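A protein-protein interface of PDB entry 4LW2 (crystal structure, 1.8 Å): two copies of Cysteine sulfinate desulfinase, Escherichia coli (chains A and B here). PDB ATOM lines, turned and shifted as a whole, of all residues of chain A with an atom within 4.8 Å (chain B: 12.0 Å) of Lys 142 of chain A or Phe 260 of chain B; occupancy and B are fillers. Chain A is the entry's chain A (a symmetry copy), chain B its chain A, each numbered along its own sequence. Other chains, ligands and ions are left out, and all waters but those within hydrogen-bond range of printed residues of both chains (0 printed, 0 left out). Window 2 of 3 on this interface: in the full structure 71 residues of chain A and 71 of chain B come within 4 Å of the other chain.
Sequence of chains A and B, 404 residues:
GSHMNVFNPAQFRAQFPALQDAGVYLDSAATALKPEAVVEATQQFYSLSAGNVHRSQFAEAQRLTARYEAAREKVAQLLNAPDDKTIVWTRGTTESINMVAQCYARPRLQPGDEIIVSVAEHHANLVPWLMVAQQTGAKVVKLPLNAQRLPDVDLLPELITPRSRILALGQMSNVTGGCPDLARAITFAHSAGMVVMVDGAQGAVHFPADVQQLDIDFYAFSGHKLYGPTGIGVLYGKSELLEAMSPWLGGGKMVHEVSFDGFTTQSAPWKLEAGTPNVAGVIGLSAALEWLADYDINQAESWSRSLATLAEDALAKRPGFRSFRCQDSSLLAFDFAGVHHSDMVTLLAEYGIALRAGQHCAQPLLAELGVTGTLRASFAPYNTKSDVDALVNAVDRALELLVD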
ATOM      1  N   VAL A 117     -17.949  25.426  25.515  1.00  0.00           N
ATOM      2  CA  VAL A 117     -18.187  24.523  24.367  1.00  0.00           C
ATOM      3  C   VAL A 117     -16.989  24.642  23.481  1.00  0.00           C
ATOM      4  O   VAL A 117     -16.610  25.769  23.187  1.00  0.00           O
ATOM      5  CB  VAL A 117     -19.493  24.929  23.594  1.00  0.00           C
ATOM      6  CG1 VAL A 117     -19.589  23.866  22.394  1.00  0.00           C
ATOM      7  CG2 VAL A 117     -20.626  24.879  24.610  1.00  0.00           C
ATOM      8  N   SER A 118     -16.327  23.530  23.097  1.00  0.00           N
ATOM      9  CA  SER A 118     -15.152  23.650  22.251  1.00  0.00           C
ATOM     10  C   SER A 118     -15.495  24.067  20.765  1.00  0.00           C
ATOM     11  O   SER A 118     -16.597  23.821  20.269  1.00  0.00           O
ATOM     12  CB  SER A 118     -14.359  22.331  22.276  1.00  0.00           C
ATOM     13  OG  SER A 118     -14.566  21.628  21.024  1.00  0.00           O
ATOM     14  N   VAL A 119     -14.520  24.721  20.102  1.00  0.00           N
ATOM     15  CA  VAL A 119     -14.625  25.176  18.753  1.00  0.00           C
ATOM     16  C   VAL A 119     -14.692  23.973  17.766  1.00  0.00           C
ATOM     17  O   VAL A 119     -15.164  24.088  16.631  1.00  0.00           O
ATOM     18  CB  VAL A 119     -13.414  26.098  18.459  1.00  0.00           C
ATOM     19  CG1 VAL A 119     -13.085  26.136  17.014  1.00  0.00           C
ATOM     20  CG2 VAL A 119     -13.800  27.506  18.880  1.00  0.00           C
ATOM     21  N   LEU A 126     -23.339  21.780  20.220  1.00  0.00           N
ATOM     22  CA  LEU A 126     -23.214  23.237  20.260  1.00  0.00           C
ATOM     23  C   LEU A 126     -24.591  23.846  20.220  1.00  0.00           C
ATOM     24  O   LEU A 126     -24.939  24.620  21.143  1.00  0.00           O
ATOM     25  CB  LEU A 126     -22.293  23.739  19.063  1.00  0.00           C
ATOM     26  CG  LEU A 126     -22.404  25.262  18.927  1.00  0.00           C
ATOM     27  CD1 LEU A 126     -21.980  26.018  20.255  1.00  0.00           C
ATOM     28  CD2 LEU A 126     -21.554  25.681  17.777  1.00  0.00           C
ATOM     29  N   LEU A 130     -26.392  26.562  22.936  1.00  0.00           N
ATOM     30  CA  LEU A 130     -26.893  27.897  22.566  1.00  0.00           C
ATOM     31  C   LEU A 130     -28.379  28.046  22.888  1.00  0.00           C
ATOM     32  O   LEU A 130     -28.845  29.115  23.329  1.00  0.00           O
ATOM     33  CB  LEU A 130     -26.710  28.159  21.053  1.00  0.00           C
ATOM     34  CG  LEU A 130     -25.264  28.209  20.593  1.00  0.00           C
ATOM     35  CD1 LEU A 130     -25.177  28.216  19.022  1.00  0.00           C
ATOM     36  CD2 LEU A 130     -24.501  29.468  21.167  1.00  0.00           C
ATOM     37  N   VAL A 140     -22.777  30.839  26.565  1.00  0.00           N
ATOM     38  CA  VAL A 140     -21.831  29.889  25.993  1.00  0.00           C
ATOM     39  C   VAL A 140     -20.475  30.598  25.859  1.00  0.00           C
ATOM     40  O   VAL A 140     -20.409  31.714  25.328  1.00  0.00           O
ATOM     41  CB  VAL A 140     -22.366  29.261  24.647  1.00  0.00           C
ATOM     42  CG1 VAL A 140     -21.209  28.451  23.936  1.00  0.00           C
ATOM     43  CG2 VAL A 140     -23.628  28.361  24.927  1.00  0.00           C
ATOM     44  N   VAL A 141     -19.442  29.959  26.358  1.00  0.00           N
ATOM     45  CA  VAL A 141     -18.065  30.403  26.351  1.00  0.00           C
ATOM     46  C   VAL A 141     -17.262  29.483  25.444  1.00  0.00           C
ATOM     47  O   VAL A 141     -17.300  28.241  25.632  1.00  0.00           O
ATOM     48  CB  VAL A 141     -17.445  30.327  27.773  1.00  0.00           C
ATOM     49  CG1 VAL A 141     -15.931  30.519  27.737  1.00  0.00           C
ATOM     50  CG2 VAL A 141     -18.116  31.352  28.693  1.00  0.00           C
ATOM     51  N   LYS A 142     -16.549  30.078  24.463  1.00  0.00           N
ATOM     52  CA  LYS A 142     -15.743  29.311  23.515  1.00  0.00           C
ATOM     53  C   LYS A 142     -14.487  28.679  24.126  1.00  0.00           C
ATOM     54  O   LYS A 142     -13.665  29.371  24.736  1.00  0.00           O
ATOM     55  CB  LYS A 142     -15.317  30.301  22.401  1.00  0.00           C
ATOM     56  CG  LYS A 142     -14.730  29.741  21.177  1.00  0.00           C
ATOM     57  CD  LYS A 142     -14.165  30.926  20.338  1.00  0.00           C
ATOM     58  CE  LYS A 142     -15.152  31.608  19.477  1.00  0.00           C
ATOM     59  NZ  LYS A 142     -14.354  32.277  18.332  1.00  0.00           N
ATOM     60  N   LEU A 143     -14.289  27.364  23.960  1.00  0.00           N
ATOM     61  CA  LEU A 143     -12.984  26.742  24.129  1.00  0.00           C
ATOM     62  C   LEU A 143     -12.262  26.664  22.772  1.00  0.00           C
ATOM     63  O   LEU A 143     -12.570  25.807  21.929  1.00  0.00           O
ATOM     64  CB  LEU A 143     -13.064  25.345  24.821  1.00  0.00           C
ATOM     65  CG  LEU A 143     -11.740  24.576  25.007  1.00  0.00           C
ATOM     66  CD1 LEU A 143     -10.720  25.396  25.886  1.00  0.00           C
ATOM     67  CD2 LEU A 143     -11.939  23.167  25.568  1.00  0.00           C
ATOM     68  N   PRO A 144     -11.215  27.500  22.572  1.00  0.00           N
ATOM     69  CA  PRO A 144     -10.445  27.475  21.327  1.00  0.00           C
ATOM     70  C   PRO A 144      -9.575  26.240  21.112  1.00  0.00           C
ATOM     71  O   PRO A 144      -9.286  25.420  22.046  1.00  0.00           O
ATOM     72  CB  PRO A 144      -9.526  28.769  21.398  1.00  0.00           C
ATOM     73  CG  PRO A 144      -9.964  29.509  22.639  1.00  0.00           C
ATOM     74  CD  PRO A 144     -10.655  28.456  23.563  1.00  0.00           C
ATOM     75  N   LEU A 159     -10.013  29.702  31.376  1.00  0.00           N
ATOM     76  CA  LEU A 159     -11.367  29.988  30.915  1.00  0.00           C
ATOM     77  C   LEU A 159     -12.440  29.635  31.939  1.00  0.00           C
ATOM     78  O   LEU A 159     -13.547  30.142  31.876  1.00  0.00           O
ATOM     79  CB  LEU A 159     -11.607  29.205  29.612  1.00  0.00           C
ATOM     80  CG  LEU A 159     -10.903  29.733  28.393  1.00  0.00           C
ATOM     81  CD1 LEU A 159     -11.267  28.762  27.301  1.00  0.00           C
ATOM     82  CD2 LEU A 159     -11.445  31.121  28.051  1.00  0.00           C
ATOM     83  N   PRO A 364     -18.186  26.042  13.013  1.00  0.00           N
ATOM     84  CA  PRO A 364     -17.184  26.880  13.748  1.00  0.00           C
ATOM     85  C   PRO A 364     -15.722  26.348  13.593  1.00  0.00           C
ATOM     86  O   PRO A 364     -14.752  27.133  13.516  1.00  0.00           O
ATOM     87  CB  PRO A 364     -17.711  26.790  15.198  1.00  0.00           C
ATOM     88  CG  PRO A 364     -19.196  26.641  15.042  1.00  0.00           C
ATOM     89  CD  PRO A 364     -19.284  25.623  13.901  1.00  0.00           C
ATOM     90  N   VAL B 255     -30.475  23.381  11.185  1.00  0.00           N
ATOM     91  CA  VAL B 255     -29.917  24.733  11.066  1.00  0.00           C
ATOM     92  C   VAL B 255     -29.447  25.015   9.639  1.00  0.00           C
ATOM     93  O   VAL B 255     -29.281  24.098   8.798  1.00  0.00           O
ATOM     94  CB  VAL B 255     -28.675  25.005  11.912  1.00  0.00           C
ATOM     95  CG1 VAL B 255     -28.954  25.204  13.373  1.00  0.00           C
ATOM     96  CG2 VAL B 255     -27.522  23.943  11.630  1.00  0.00           C
ATOM     97  N   HIS B 256     -29.358  26.316   9.318  1.00  0.00           N
ATOM     98  CA  HIS B 256     -28.580  26.736   8.150  1.00  0.00           C
ATOM     99  C   HIS B 256     -27.157  27.113   8.627  1.00  0.00           C
ATOM    100  O   HIS B 256     -26.214  26.382   8.435  1.00  0.00           O
ATOM    101  CB  HIS B 256     -29.312  27.885   7.422  1.00  0.00           C
ATOM    102  CG  HIS B 256     -30.385  27.392   6.475  1.00  0.00           C
ATOM    103  ND1 HIS B 256     -30.089  26.626   5.352  1.00  0.00           N
ATOM    104  CD2 HIS B 256     -31.730  27.539   6.498  1.00  0.00           C
ATOM    105  CE1 HIS B 256     -31.220  26.330   4.728  1.00  0.00           C
ATOM    106  NE2 HIS B 256     -32.229  26.867   5.405  1.00  0.00           N
ATOM    107  N   GLU B 257     -27.019  28.264   9.257  1.00  0.00           N
ATOM    108  CA  GLU B 257     -25.751  28.738   9.809  1.00  0.00           C
ATOM    109  C   GLU B 257     -25.695  28.610  11.315  1.00  0.00           C
ATOM    110  O   GLU B 257     -26.713  28.671  11.968  1.00  0.00           O
ATOM    111  CB  GLU B 257     -25.536  30.212   9.445  1.00  0.00           C
ATOM    112  CG  GLU B 257     -25.318  30.440   7.956  1.00  0.00           C
ATOM    113  CD  GLU B 257     -26.619  30.394   7.110  1.00  0.00           C
ATOM    114  OE1 GLU B 257     -27.621  31.023   7.505  1.00  0.00           O
ATOM    115  OE2 GLU B 257     -26.575  29.809   5.985  1.00  0.00           O
ATOM    116  N   VAL B 258     -24.500  28.316  11.846  1.00  0.00           N
ATOM    117  CA  VAL B 258     -24.313  28.129  13.270  1.00  0.00           C
ATOM    118  C   VAL B 258     -22.999  28.811  13.636  1.00  0.00           C
ATOM    119  O   VAL B 258     -21.981  28.575  12.999  1.00  0.00           O
ATOM    120  CB  VAL B 258     -24.082  26.564  13.709  1.00  0.00           C
ATOM    121  CG1 VAL B 258     -23.944  26.503  15.311  1.00  0.00           C
ATOM    122  CG2 VAL B 258     -25.176  25.716  13.266  1.00  0.00           C
ATOM    123  N   SER B 259     -22.985  29.626  14.717  1.00  0.00           N
ATOM    124  CA  SER B 259     -21.695  30.113  15.200  1.00  0.00           C
ATOM    125  C   SER B 259     -21.826  30.191  16.725  1.00  0.00           C
ATOM    126  O   SER B 259     -22.880  29.944  17.254  1.00  0.00           O
ATOM    127  CB  SER B 259     -21.404  31.546  14.684  1.00  0.00           C
ATOM    128  OG  SER B 259     -22.377  32.409  15.296  1.00  0.00           O
ATOM    129  N   PHE B 260     -20.766  30.628  17.396  1.00  0.00           N
ATOM    130  CA  PHE B 260     -20.864  30.921  18.811  1.00  0.00           C
ATOM    131  C   PHE B 260     -21.802  32.036  19.225  1.00  0.00           C
ATOM    132  O   PHE B 260     -22.085  32.218  20.415  1.00  0.00           O
ATOM    133  CB  PHE B 260     -19.462  31.030  19.445  1.00  0.00           C
ATOM    134  CG  PHE B 260     -18.863  29.698  19.727  1.00  0.00           C
ATOM    135  CD1 PHE B 260     -18.243  28.935  18.698  1.00  0.00           C
ATOM    136  CD2 PHE B 260     -18.974  29.128  21.016  1.00  0.00           C
ATOM    137  CE1 PHE B 260     -17.692  27.632  18.939  1.00  0.00           C
ATOM    138  CE2 PHE B 260     -18.430  27.821  21.230  1.00  0.00           C
ATOM    139  CZ  PHE B 260     -17.859  27.072  20.197  1.00  0.00           C
ATOM    140  N   ASP B 261     -22.328  32.761  18.250  1.00  0.00           N
ATOM    141  CA  ASP B 261     -23.223  33.878  18.547  1.00  0.00           C
ATOM    142  C   ASP B 261     -24.664  33.577  18.260  1.00  0.00           C
ATOM    143  O   ASP B 261     -25.521  34.411  18.488  1.00  0.00           O
ATOM    144  CB  ASP B 261     -22.756  35.115  17.730  1.00  0.00           C
ATOM    145  CG  ASP B 261     -21.413  35.595  18.189  1.00  0.00           C
ATOM    146  OD1 ASP B 261     -21.288  35.799  19.414  1.00  0.00           O
ATOM    147  OD2 ASP B 261     -20.464  35.656  17.403  1.00  0.00           O
ATOM    148  N   GLY B 262     -24.963  32.405  17.693  1.00  0.00           N
ATOM    149  CA  GLY B 262     -26.311  32.077  17.430  1.00  0.00           C
ATOM    150  C   GLY B 262     -26.449  31.228  16.184  1.00  0.00           C
ATOM    151  O   GLY B 262     -25.451  30.819  15.618  1.00  0.00           O
ATOM    152  N   PHE B 263     -27.691  30.976  15.766  1.00  0.00           N
ATOM    153  CA  PHE B 263     -27.916  30.086  14.618  1.00  0.00           C
ATOM    154  C   PHE B 263     -29.157  30.541  13.889  1.00  0.00           C
ATOM    155  O   PHE B 263     -30.042  31.229  14.461  1.00  0.00           O
ATOM    156  CB  PHE B 263     -28.075  28.576  15.045  1.00  0.00           C
ATOM    157  CG  PHE B 263     -29.167  28.323  16.066  1.00  0.00           C
ATOM    158  CD1 PHE B 263     -30.502  28.041  15.684  1.00  0.00           C
ATOM    159  CD2 PHE B 263     -28.862  28.369  17.433  1.00  0.00           C
ATOM    160  CE1 PHE B 263     -31.501  27.792  16.735  1.00  0.00           C
ATOM    161  CE2 PHE B 263     -29.775  28.193  18.428  1.00  0.00           C
ATOM    162  CZ  PHE B 263     -31.134  27.882  18.110  1.00  0.00           C
ATOM    163  N   THR B 264     -29.246  30.135  12.623  1.00  0.00           N
ATOM    164  CA  THR B 264     -30.435  30.374  11.827  1.00  0.00           C
ATOM    165  C   THR B 264     -30.994  28.981  11.491  1.00  0.00           C
ATOM    166  O   THR B 264     -30.229  28.010  11.328  1.00  0.00           O
ATOM    167  CB  THR B 264     -30.111  31.098  10.523  1.00  0.00           C
ATOM    168  OG1 THR B 264     -29.090  30.351   9.847  1.00  0.00           O
ATOM    169  CG2 THR B 264     -29.586  32.498  10.854  1.00  0.00           C
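Of the 10 printed residues of chain B, 3 touch a printed residue of chain A. Hydrophobic or aromatic side chains of chain B that line the printed part of chain A: Val 258 and Phe 260. Along chain B the printed residues that touch a printed residue of chain A span positions 258 to 260. Of the 12 printed residues of chain A, 8 touch a printed residue of chain B. Printed residues of chain A that touch a printed residue of chain B: Val 117, Ser 118, Val 119, Leu 126, Leu 130, Val 140, Lys 142 and Pro 364. Hydrophobic or aromatic side chains of chain A that line the printed part of chain B: Val 117, Val 119, Leu 126, Leu 130, Val 140 and Pro 364.
The backbone carbonyl oxygen of Val 141 of chain A lies within hydrogen-bond range of the backbone NH of Val 117 of chain A (2.9 Å). N of Val 119 of chain A lies within hydrogen-bond range of O of Leu 143 of chain A. N of Leu 143 of chain A sits at hydrogen-bond distance from O of Val 117 of chain A, 2.9 Å away. The side-chain hydroxyl of Ser 259 of chain B is in hydrogen-bond range of the backbone NH of Asp 261 of chain B (3.0 Å). The side-chain hydroxyl of Ser 259 of chain B lies within hydrogen-bond range of the backbone carbonyl oxygen of Gly 262 of chain B (3.5 Å).
Val 117 of chain A touches Phe 260 of chain B (O to CE2, 3.4 Å). O of Ser 118 of chain A touches CZ of Phe 260 of chain B, 3.5 Å away. Phe 260 of chain B touches Val 119 of chain A (CE1 to CG2, 3.9 Å). CD2 of Leu 126 of chain A touches CG1 of Val 258 of chain B (3.5 Å). Ser 259 of chain B touches Leu 130 of chain A. Phe 260 of chain B touches Leu 130 of chain A (O to CD2, 3.7 Å). Val 140 of chain A touches Phe 260 of chain B. Phe 260 of chain B touches Lys 142 of chain A. Val 258 of chain B touches Pro 364 of chain A. CE1 of Phe 260 of chain B touches CB of Pro 364 of chain A (3.8 Å).
Val 117 of chain A touches just one residue of chain B: Phe 260. Ser 118 of chain A touches just one residue of chain B: Phe 260 (3.5 Å). Printed residues of chain B within 4 Å of Val 119 of chain A: Phe 260. Leu 126 of chain A touches just one residue of chain B: Val 258 (3.5 Å). Val 140 of chain A touches just one residue of chain B: Phe 260 (3.7 Å). No residue of chain B comes within 4 Å of Val 141 of chain A. Printed residues of chain B within 4 Å of Lys 142 of chain A: Phe 260. Leu 143 of chain A touches none of the printed residues of chain B. Pro 144 of chain A touches none of the printed residues of chain B. Of chain B, only Val 258 and Phe 260 come within 4 Å of Pro 364 of chain A. Of the printed residues of chain A, Val 258 of chain B touches Leu 126 (3.5 Å) and Pro 364 (3.96 Å). Printed residues of chain A within 4 Å of Ser 259 of chain B: Leu 130 (3.4 Å). Of chain A, only Val 117 (3.4 Å), Ser 118 (3.5 Å), Val 119 (3.9 Å), Leu 130 (3.7 Å), Val 140 (3.7 Å), Lys 142 (3.8 Å) and Pro 364 (3.8 Å) come within 4 Å of Phe 260 of chain B. The nearest printed residue of chain A that does not touch Val 258 of chain B is Leu 130 of chain A (4.3 Å).
No position is printed for both chains. Of the 10 pairs that touch across the chains among the printed residues, none has its exchanged pair printed and touching as well.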
